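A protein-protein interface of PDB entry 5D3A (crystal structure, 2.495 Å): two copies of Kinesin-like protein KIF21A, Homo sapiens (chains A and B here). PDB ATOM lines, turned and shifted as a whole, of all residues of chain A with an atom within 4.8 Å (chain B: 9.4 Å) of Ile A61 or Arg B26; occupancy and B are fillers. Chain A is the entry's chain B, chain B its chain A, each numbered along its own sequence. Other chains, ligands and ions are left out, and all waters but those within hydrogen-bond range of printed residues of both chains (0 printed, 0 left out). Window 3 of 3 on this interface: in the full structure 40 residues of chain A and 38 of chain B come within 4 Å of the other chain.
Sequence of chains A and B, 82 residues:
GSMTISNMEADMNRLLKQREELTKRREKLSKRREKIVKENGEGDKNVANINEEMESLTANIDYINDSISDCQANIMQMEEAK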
ATOM      1  N   MET A  54       5.953   9.574  -8.371  1.00  0.00           N
ATOM      2  CA  MET A  54       4.777   9.663  -9.229  1.00  0.00           C
ATOM      3  C   MET A  54       3.854  10.790  -8.767  1.00  0.00           C
ATOM      4  O   MET A  54       3.292  11.515  -9.587  1.00  0.00           O
ATOM      5  CB  MET A  54       4.018   8.332  -9.247  1.00  0.00           C
ATOM      6  CG  MET A  54       4.812   7.172  -9.835  1.00  0.00           C
ATOM      7  SD  MET A  54       3.820   5.693 -10.133  1.00  0.00           S
ATOM      8  CE  MET A  54       2.898   6.184 -11.586  1.00  0.00           C
ATOM      9  N   LEU A  57       5.221  13.935 -10.266  1.00  0.00           N
ATOM     10  CA  LEU A  57       4.943  13.967 -11.697  1.00  0.00           C
ATOM     11  C   LEU A  57       3.491  14.348 -11.945  1.00  0.00           C
ATOM     12  O   LEU A  57       3.189  15.124 -12.852  1.00  0.00           O
ATOM     13  CB  LEU A  57       5.248  12.615 -12.345  1.00  0.00           C
ATOM     14  CG  LEU A  57       6.702  12.141 -12.271  1.00  0.00           C
ATOM     15  CD1 LEU A  57       6.837  10.752 -12.869  1.00  0.00           C
ATOM     16  CD2 LEU A  57       7.635  13.111 -12.969  1.00  0.00           C
ATOM     17  N   THR A  58       2.593  13.806 -11.128  1.00  0.00           N
ATOM     18  CA  THR A  58       1.171  14.093 -11.264  1.00  0.00           C
ATOM     19  C   THR A  58       0.911  15.570 -11.004  1.00  0.00           C
ATOM     20  O   THR A  58       0.007  16.163 -11.592  1.00  0.00           O
ATOM     21  CB  THR A  58       0.327  13.237 -10.300  1.00  0.00           C
ATOM     22  OG1 THR A  58       0.483  11.850 -10.630  1.00  0.00           O
ATOM     23  CG2 THR A  58      -1.147  13.610 -10.389  1.00  0.00           C
ATOM     24  N   ALA A  59       1.712  16.166 -10.130  1.00  0.00           N
ATOM     25  CA  ALA A  59       1.561  17.576  -9.805  1.00  0.00           C
ATOM     26  C   ALA A  59       2.017  18.439 -10.969  1.00  0.00           C
ATOM     27  O   ALA A  59       1.331  19.383 -11.363  1.00  0.00           O
ATOM     28  CB  ALA A  59       2.344  17.917  -8.551  1.00  0.00           C
ATOM     29  N   ASN A  60       3.177  18.106 -11.522  1.00  0.00           N
ATOM     30  CA  ASN A  60       3.756  18.878 -12.613  1.00  0.00           C
ATOM     31  C   ASN A  60       3.012  18.634 -13.920  1.00  0.00           C
ATOM     32  O   ASN A  60       2.791  19.561 -14.695  1.00  0.00           O
ATOM     33  CB  ASN A  60       5.234  18.535 -12.771  1.00  0.00           C
ATOM     34  CG  ASN A  60       6.040  18.874 -11.536  1.00  0.00           C
ATOM     35  OD1 ASN A  60       5.790  19.887 -10.877  1.00  0.00           O
ATOM     36  ND2 ASN A  60       7.004  18.024 -11.205  1.00  0.00           N
ATOM     37  N   ILE A  61       2.633  17.383 -14.162  1.00  0.00           N
ATOM     38  CA  ILE A  61       1.812  17.044 -15.319  1.00  0.00           C
ATOM     39  C   ILE A  61       0.556  17.917 -15.323  1.00  0.00           C
ATOM     40  O   ILE A  61       0.242  18.559 -16.324  1.00  0.00           O
ATOM     41  CB  ILE A  61       1.463  15.540 -15.323  1.00  0.00           C
ATOM     42  CG1 ILE A  61       2.700  14.723 -15.697  1.00  0.00           C
ATOM     43  CG2 ILE A  61       0.341  15.237 -16.307  1.00  0.00           C
ATOM     44  CD1 ILE A  61       2.589  13.250 -15.370  1.00  0.00           C
ATOM     45  N   ASP A  62      -0.157  17.949 -14.203  1.00  0.00           N
ATOM     46  CA  ASP A  62      -1.346  18.786 -14.087  1.00  0.00           C
ATOM     47  C   ASP A  62      -1.001  20.237 -14.377  1.00  0.00           C
ATOM     48  O   ASP A  62      -1.747  20.937 -15.056  1.00  0.00           O
ATOM     49  CB  ASP A  62      -1.965  18.667 -12.692  1.00  0.00           C
ATOM     50  CG  ASP A  62      -2.819  17.420 -12.531  1.00  0.00           C
ATOM     51  OD1 ASP A  62      -3.280  16.873 -13.555  1.00  0.00           O
ATOM     52  OD2 ASP A  62      -3.040  16.993 -11.377  1.00  0.00           O
ATOM     53  N   TYR A  63       0.135  20.684 -13.854  1.00  0.00           N
ATOM     54  CA  TYR A  63       0.564  22.067 -14.025  1.00  0.00           C
ATOM     55  C   TYR A  63       0.871  22.388 -15.484  1.00  0.00           C
ATOM     56  O   TYR A  63       0.427  23.409 -16.005  1.00  0.00           O
ATOM     57  CB  TYR A  63       1.795  22.352 -13.167  1.00  0.00           C
ATOM     58  CG  TYR A  63       2.489  23.638 -13.538  1.00  0.00           C
ATOM     59  CD1 TYR A  63       1.845  24.858 -13.400  1.00  0.00           C
ATOM     60  CD2 TYR A  63       3.786  23.633 -14.025  1.00  0.00           C
ATOM     61  CE1 TYR A  63       2.470  26.037 -13.739  1.00  0.00           C
ATOM     62  CE2 TYR A  63       4.423  24.812 -14.367  1.00  0.00           C
ATOM     63  CZ  TYR A  63       3.759  26.011 -14.220  1.00  0.00           C
ATOM     64  OH  TYR A  63       4.387  27.188 -14.557  1.00  0.00           O
ATOM     65  N   ILE A  64       1.642  21.520 -16.134  1.00  0.00           N
ATOM     66  CA  ILE A  64       1.978  21.700 -17.539  1.00  0.00           C
ATOM     67  C   ILE A  64       0.701  21.739 -18.364  1.00  0.00           C
ATOM     68  O   ILE A  64       0.556  22.583 -19.244  1.00  0.00           O
ATOM     69  CB  ILE A  64       2.927  20.588 -18.034  1.00  0.00           C
ATOM     70  CG1 ILE A  64       4.286  20.679 -17.331  1.00  0.00           C
ATOM     71  CG2 ILE A  64       3.117  20.660 -19.542  1.00  0.00           C
ATOM     72  CD1 ILE A  64       5.046  21.974 -17.573  1.00  0.00           C
ATOM     73  N   ASN A  65      -0.227  20.833 -18.078  1.00  0.00           N
ATOM     74  CA  ASN A  65      -1.494  20.800 -18.800  1.00  0.00           C
ATOM     75  C   ASN A  65      -2.264  22.100 -18.592  1.00  0.00           C
ATOM     76  O   ASN A  65      -2.823  22.658 -19.536  1.00  0.00           O
ATOM     77  CB  ASN A  65      -2.339  19.603 -18.358  1.00  0.00           C
ATOM     78  CG  ASN A  65      -2.053  18.354 -19.172  1.00  0.00           C
ATOM     79  OD1 ASN A  65      -1.628  18.434 -20.325  1.00  0.00           O
ATOM     80  ND2 ASN A  65      -2.293  17.191 -18.578  1.00  0.00           N
ATOM     81  N   LEU B  15       5.826  22.818 -24.359  1.00  0.00           N
ATOM     82  CA  LEU B  15       4.991  22.308 -23.279  1.00  0.00           C
ATOM     83  C   LEU B  15       4.526  20.894 -23.601  1.00  0.00           C
ATOM     84  O   LEU B  15       4.364  20.067 -22.704  1.00  0.00           O
ATOM     85  CB  LEU B  15       3.781  23.212 -23.049  1.00  0.00           C
ATOM     86  CG  LEU B  15       4.046  24.613 -22.503  1.00  0.00           C
ATOM     87  CD1 LEU B  15       2.778  25.448 -22.571  1.00  0.00           C
ATOM     88  CD2 LEU B  15       4.556  24.540 -21.074  1.00  0.00           C
ATOM     89  N   GLN B  18       7.519  18.747 -22.909  1.00  0.00           N
ATOM     90  CA  GLN B  18       7.566  18.554 -21.464  1.00  0.00           C
ATOM     91  C   GLN B  18       6.490  17.574 -21.007  1.00  0.00           C
ATOM     92  O   GLN B  18       6.742  16.702 -20.179  1.00  0.00           O
ATOM     93  CB  GLN B  18       7.389  19.890 -20.747  1.00  0.00           C
ATOM     94  CG  GLN B  18       8.571  20.827 -20.880  1.00  0.00           C
ATOM     95  CD  GLN B  18       8.382  22.106 -20.087  1.00  0.00           C
ATOM     96  OE1 GLN B  18       7.803  23.075 -20.578  1.00  0.00           O
ATOM     97  NE2 GLN B  18       8.872  22.117 -18.851  1.00  0.00           N
ATOM     98  N   ARG B  19       5.290  17.726 -21.556  1.00  0.00           N
ATOM     99  CA  ARG B  19       4.171  16.849 -21.232  1.00  0.00           C
ATOM    100  C   ARG B  19       4.455  15.425 -21.700  1.00  0.00           C
ATOM    101  O   ARG B  19       3.949  14.462 -21.127  1.00  0.00           O
ATOM    102  CB  ARG B  19       2.888  17.381 -21.872  1.00  0.00           C
ATOM    103  CG  ARG B  19       1.602  16.758 -21.348  1.00  0.00           C
ATOM    104  CD  ARG B  19       1.155  15.558 -22.168  1.00  0.00           C
ATOM    105  NE  ARG B  19       1.019  15.866 -23.589  1.00  0.00           N
ATOM    106  CZ  ARG B  19       0.011  16.554 -24.118  1.00  0.00           C
ATOM    107  NH1 ARG B  19      -0.959  17.028 -23.344  1.00  0.00           N
ATOM    108  NH2 ARG B  19      -0.021  16.775 -25.424  1.00  0.00           N
ATOM    109  N   GLU B  20       5.275  15.301 -22.739  1.00  0.00           N
ATOM    110  CA  GLU B  20       5.652  13.997 -23.277  1.00  0.00           C
ATOM    111  C   GLU B  20       6.727  13.341 -22.411  1.00  0.00           C
ATOM    112  O   GLU B  20       6.763  12.118 -22.270  1.00  0.00           O
ATOM    113  CB  GLU B  20       6.152  14.144 -24.718  1.00  0.00           C
ATOM    114  CG  GLU B  20       6.622  12.849 -25.367  1.00  0.00           C
ATOM    115  CD  GLU B  20       7.296  13.082 -26.707  1.00  0.00           C
ATOM    116  OE1 GLU B  20       7.175  14.202 -27.249  1.00  0.00           O
ATOM    117  OE2 GLU B  20       7.952  12.149 -27.218  1.00  0.00           O
ATOM    118  N   GLU B  21       7.602  14.157 -21.836  1.00  0.00           N
ATOM    119  CA  GLU B  21       8.688  13.647 -21.007  1.00  0.00           C
ATOM    120  C   GLU B  21       8.154  13.107 -19.683  1.00  0.00           C
ATOM    121  O   GLU B  21       8.658  12.113 -19.161  1.00  0.00           O
ATOM    122  CB  GLU B  21       9.725  14.743 -20.754  1.00  0.00           C
ATOM    123  CG  GLU B  21      10.480  15.173 -22.006  1.00  0.00           C
ATOM    124  CD  GLU B  21      11.208  16.494 -21.831  1.00  0.00           C
ATOM    125  OE1 GLU B  21      11.990  16.869 -22.733  1.00  0.00           O
ATOM    126  OE2 GLU B  21      10.995  17.158 -20.793  1.00  0.00           O
ATOM    127  N   LEU B  22       7.128  13.764 -19.153  1.00  0.00           N
ATOM    128  CA  LEU B  22       6.560  13.397 -17.860  1.00  0.00           C
ATOM    129  C   LEU B  22       5.737  12.114 -17.938  1.00  0.00           C
ATOM    130  O   LEU B  22       5.973  11.172 -17.183  1.00  0.00           O
ATOM    131  CB  LEU B  22       5.686  14.534 -17.323  1.00  0.00           C
ATOM    132  CG  LEU B  22       6.379  15.882 -17.108  1.00  0.00           C
ATOM    133  CD1 LEU B  22       5.346  16.973 -16.896  1.00  0.00           C
ATOM    134  CD2 LEU B  22       7.340  15.824 -15.930  1.00  0.00           C
ATOM    135  N   THR B  23       4.769  12.085 -18.848  1.00  0.00           N
ATOM    136  CA  THR B  23       3.857  10.949 -18.958  1.00  0.00           C
ATOM    137  C   THR B  23       4.609   9.642 -19.184  1.00  0.00           C
ATOM    138  O   THR B  23       4.279   8.620 -18.583  1.00  0.00           O
ATOM    139  CB  THR B  23       2.845  11.144 -20.100  1.00  0.00           C
ATOM    140  OG1 THR B  23       3.543  11.352 -21.334  1.00  0.00           O
ATOM    141  CG2 THR B  23       1.939  12.335 -19.815  1.00  0.00           C
ATOM    142  N   LYS B  24       5.619   9.671 -20.047  1.00  0.00           N
ATOM    143  CA  LYS B  24       6.412   8.474 -20.302  1.00  0.00           C
ATOM    144  C   LYS B  24       7.215   8.105 -19.060  1.00  0.00           C
ATOM    145  O   LYS B  24       7.432   6.927 -18.778  1.00  0.00           O
ATOM    146  CB  LYS B  24       7.348   8.671 -21.497  1.00  0.00           C
ATOM    147  CG  LYS B  24       8.171   7.429 -21.822  1.00  0.00           C
ATOM    148  CD  LYS B  24       8.871   7.531 -23.170  1.00  0.00           C
ATOM    149  CE  LYS B  24       9.621   6.244 -23.493  1.00  0.00           C
ATOM    150  NZ  LYS B  24      10.274   6.282 -24.833  1.00  0.00           N
ATOM    151  N   ARG B  25       7.654   9.114 -18.316  1.00  0.00           N
ATOM    152  CA  ARG B  25       8.390   8.872 -17.083  1.00  0.00           C
ATOM    153  C   ARG B  25       7.446   8.335 -16.016  1.00  0.00           C
ATOM    154  O   ARG B  25       7.825   7.486 -15.210  1.00  0.00           O
ATOM    155  CB  ARG B  25       9.080  10.146 -16.591  1.00  0.00           C
ATOM    156  CG  ARG B  25       9.665  10.014 -15.192  1.00  0.00           C
ATOM    157  CD  ARG B  25      10.675  11.109 -14.880  1.00  0.00           C
ATOM    158  NE  ARG B  25      10.797  11.353 -13.442  1.00  0.00           N
ATOM    159  CZ  ARG B  25      11.340  10.501 -12.575  1.00  0.00           C
ATOM    160  NH1 ARG B  25      11.810   9.332 -12.986  1.00  0.00           N
ATOM    161  NH2 ARG B  25      11.405  10.818 -11.288  1.00  0.00           N
ATOM    162  N   ARG B  26       6.213   8.828 -16.016  1.00  0.00           N
ATOM    163  CA  ARG B  26       5.219   8.348 -15.069  1.00  0.00           C
ATOM    164  C   ARG B  26       4.761   6.945 -15.458  1.00  0.00           C
ATOM    165  O   ARG B  26       4.217   6.211 -14.635  1.00  0.00           O
ATOM    166  CB  ARG B  26       4.025   9.301 -14.999  1.00  0.00           C
ATOM    167  CG  ARG B  26       3.030   8.946 -13.903  1.00  0.00           C
ATOM    168  CD  ARG B  26       1.950  10.002 -13.753  1.00  0.00           C
ATOM    169  NE  ARG B  26       1.184  10.177 -14.984  1.00  0.00           N
ATOM    170  CZ  ARG B  26       0.088  10.923 -15.084  1.00  0.00           C
ATOM    171  NH1 ARG B  26      -0.538  11.023 -16.250  1.00  0.00           N
ATOM    172  NH2 ARG B  26      -0.383  11.567 -14.023  1.00  0.00           N
ATOM    173  N   GLU B  27       4.985   6.575 -16.715  1.00  0.00           N
ATOM    174  CA  GLU B  27       4.655   5.232 -17.183  1.00  0.00           C
ATOM    175  C   GLU B  27       5.744   4.239 -16.791  1.00  0.00           C
ATOM    176  O   GLU B  27       5.450   3.156 -16.291  1.00  0.00           O
ATOM    177  CB  GLU B  27       4.456   5.224 -18.700  1.00  0.00           C
ATOM    178  CG  GLU B  27       3.019   4.980 -19.138  1.00  0.00           C
ATOM    179  CD  GLU B  27       2.537   3.570 -18.830  1.00  0.00           C
ATOM    180  OE1 GLU B  27       2.019   3.344 -17.716  1.00  0.00           O
ATOM    181  OE2 GLU B  27       2.672   2.690 -19.705  1.00  0.00           O
ATOM    182  N   LYS B  28       7.001   4.609 -17.018  1.00  0.00           N
ATOM    183  CA  LYS B  28       8.122   3.730 -16.697  1.00  0.00           C
ATOM    184  C   LYS B  28       8.094   3.341 -15.225  1.00  0.00           C
ATOM    185  O   LYS B  28       8.298   2.180 -14.872  1.00  0.00           O
ATOM    186  CB  LYS B  28       9.455   4.401 -17.040  1.00  0.00           C
ATOM    187  CG  LYS B  28       9.719   4.528 -18.535  1.00  0.00           C
ATOM    188  CD  LYS B  28      11.171   4.882 -18.823  1.00  0.00           C
ATOM    189  CE  LYS B  28      11.469   4.837 -20.315  1.00  0.00           C
ATOM    190  NZ  LYS B  28      12.915   5.042 -20.606  1.00  0.00           N
ATOM    191  N   LEU B  29       7.834   4.320 -14.368  1.00  0.00           N
ATOM    192  CA  LEU B  29       7.718   4.064 -12.941  1.00  0.00           C
ATOM    193  C   LEU B  29       6.515   3.169 -12.656  1.00  0.00           C
ATOM    194  O   LEU B  29       6.600   2.228 -11.866  1.00  0.00           O
ATOM    195  CB  LEU B  29       7.600   5.378 -12.170  1.00  0.00           C
ATOM    196  CG  LEU B  29       8.922   6.033 -11.771  1.00  0.00           C
ATOM    197  CD1 LEU B  29       9.850   6.188 -12.966  1.00  0.00           C
ATOM    198  CD2 LEU B  29       8.661   7.381 -11.122  1.00  0.00           C
ATOM    199  N   SER B  30       5.396   3.464 -13.308  1.00  0.00           N
ATOM    200  CA  SER B  30       4.177   2.690 -13.116  1.00  0.00           C
ATOM    201  C   SER B  30       4.412   1.226 -13.471  1.00  0.00           C
ATOM    202  O   SER B  30       3.784   0.330 -12.912  1.00  0.00           O
ATOM    203  CB  SER B  30       3.039   3.262 -13.961  1.00  0.00           C
ATOM    204  OG  SER B  30       1.865   2.483 -13.826  1.00  0.00           O
ATOM    205  N   LYS B  31       5.323   0.994 -14.408  1.00  0.00           N
ATOM    206  CA  LYS B  31       5.663  -0.356 -14.830  1.00  0.00           C
ATOM    207  C   LYS B  31       6.553  -1.016 -13.786  1.00  0.00           C
ATOM    208  O   LYS B  31       6.288  -2.135 -13.348  1.00  0.00           O
ATOM    209  CB  LYS B  31       6.369  -0.334 -16.187  1.00  0.00           C
ATOM    210  CG  LYS B  31       5.616   0.426 -17.272  1.00  0.00           C
ATOM    211  CD  LYS B  31       5.198  -0.486 -18.410  1.00  0.00           C
ATOM    212  CE  LYS B  31       4.590   0.303 -19.558  1.00  0.00           C
ATOM    213  NZ  LYS B  31       4.179  -0.574 -20.689  1.00  0.00           N
ATOM    214  N   ARG B  32       7.608  -0.306 -13.394  1.00  0.00           N
ATOM    215  CA  ARG B  32       8.548  -0.788 -12.390  1.00  0.00           C
ATOM    216  C   ARG B  32       7.825  -1.171 -11.105  1.00  0.00           C
ATOM    217  O   ARG B  32       8.075  -2.227 -10.522  1.00  0.00           O
ATOM    218  CB  ARG B  32       9.595   0.285 -12.097  1.00  0.00           C
ATOM    219  CG  ARG B  32      10.748  -0.185 -11.222  1.00  0.00           C
ATOM    220  CD  ARG B  32      11.734   0.945 -10.950  1.00  0.00           C
ATOM    221  NE  ARG B  32      12.175   1.598 -12.181  1.00  0.00           N
ATOM    222  CZ  ARG B  32      12.980   2.656 -12.224  1.00  0.00           C
ATOM    223  NH1 ARG B  32      13.444   3.192 -11.102  1.00  0.00           N
ATOM    224  NH2 ARG B  32      13.322   3.180 -13.394  1.00  0.00           N
ATOM    225  N   ARG B  33       6.926  -0.296 -10.673  1.00  0.00           N
ATOM    226  CA  ARG B  33       6.160  -0.502  -9.455  1.00  0.00           C
ATOM    227  C   ARG B  33       5.349  -1.789  -9.523  1.00  0.00           C
ATOM    228  O   ARG B  33       5.187  -2.482  -8.521  1.00  0.00           O
ATOM    229  CB  ARG B  33       5.233   0.690  -9.215  1.00  0.00           C
ATOM    230  CG  ARG B  33       4.409   0.597  -7.952  1.00  0.00           C
ATOM    231  CD  ARG B  33       3.607   1.870  -7.725  1.00  0.00           C
ATOM    232  NE  ARG B  33       2.694   2.157  -8.829  1.00  0.00           N
ATOM    233  CZ  ARG B  33       1.793   3.137  -8.825  1.00  0.00           C
ATOM    234  NH1 ARG B  33       1.671   3.931  -7.769  1.00  0.00           N
ATOM    235  NH2 ARG B  33       1.007   3.321  -9.876  1.00  0.00           N
ATOM    236  N   GLU B  34       4.841  -2.102 -10.709  1.00  0.00           N
ATOM    237  CA  GLU B  34       3.987  -3.269 -10.892  1.00  0.00           C
ATOM    238  C   GLU B  34       4.798  -4.560 -10.848  1.00  0.00           C
ATOM    239  O   GLU B  34       4.295  -5.602 -10.431  1.00  0.00           O
ATOM    240  CB  GLU B  34       3.224  -3.171 -12.215  1.00  0.00           C
ATOM    241  CG  GLU B  34       2.379  -4.397 -12.539  1.00  0.00           C
ATOM    242  CD  GLU B  34       1.401  -4.748 -11.435  1.00  0.00           C
ATOM    243  OE1 GLU B  34       0.890  -3.819 -10.772  1.00  0.00           O
ATOM    244  OE2 GLU B  34       1.146  -5.953 -11.225  1.00  0.00           O
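Hydrophobic or aromatic side chains of chain A that line the printed part of chain B: Met A54, Leu A57, Ile A61 and Ile A64.
Along chain A the printed residues that touch a printed residue of chain B span positions 54 to 65.
Of the 18 printed residues of chain B, 7 touch a printed residue of chain A.
Hydrophobic or aromatic side chains of chain B within 4 Å of the printed part of chain A: Leu B22.
Among the printed residues, no Asp or Glu carboxylate lies within 4 Å of a Lys or Arg side-chain nitrogen of the other chain.
Of chain B, only Leu B22 (3.4 Å) and Arg B26 (3.4 Å) come within 4 Å of Ile A61.
Thr A58 touches one residue of chain B.
No residue of chain B comes within 4 Å of Asn A60.
Printed residues of chain B within 4 Å of Leu A57: Arg B25 (3.6 Å) and Arg B26 (3.6 Å).
Printed residues of chain A within 4 Å of Leu B15: Ile A64.
Of the printed residues of chain B, Met A54 touches Arg B26 (3.3 Å), Ser B30 (3.8 Å) and Arg B33 (3.5 Å).
Of the printed residues of chain A, Ser B30 touches Met A54.
Glu B20 touches none of the printed residues of chain A.
The nearest printed residue of chain A that does not touch Arg B26 is Asp A62 (6.1 Å).
Among the printed residues, merely in contact across the chains: Met A54 with Arg B26 (3.3 Å), Ile A61 with Arg B26 (3.4 Å), Ile A61 with Leu B22 (3.4 Å), Ile A64 with Leu B15 (3.5 Å), Thr A58 with Arg B26 (3.5 Å), Leu A57 with Arg B26 (3.6 Å), Leu A57 with Arg B25 (3.6 Å), Met A54 with Ser B30 (3.8 Å) and Ile A64 with Leu B22 (3.9 Å).
The backbone carbonyl oxygen (O) of Arg B19 lies within hydrogen-bond range of the side-chain hydroxyl (OG1) of Thr B23.
The backbone carbonyl oxygen (O) of Met A54 lies within hydrogen-bond range of the side-chain hydroxyl (OG1) of Thr A58 (3.0 Å).
No position is printed for both chains.
The side-chain amide oxygen (OD1) of Asn A65 sits at hydrogen-bond distance from the guanidinium group (NH1) of Arg B19.
The guanidinium group of Arg B33 lies close to the side-chain sulfur of Met A54 (3.6 Å).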
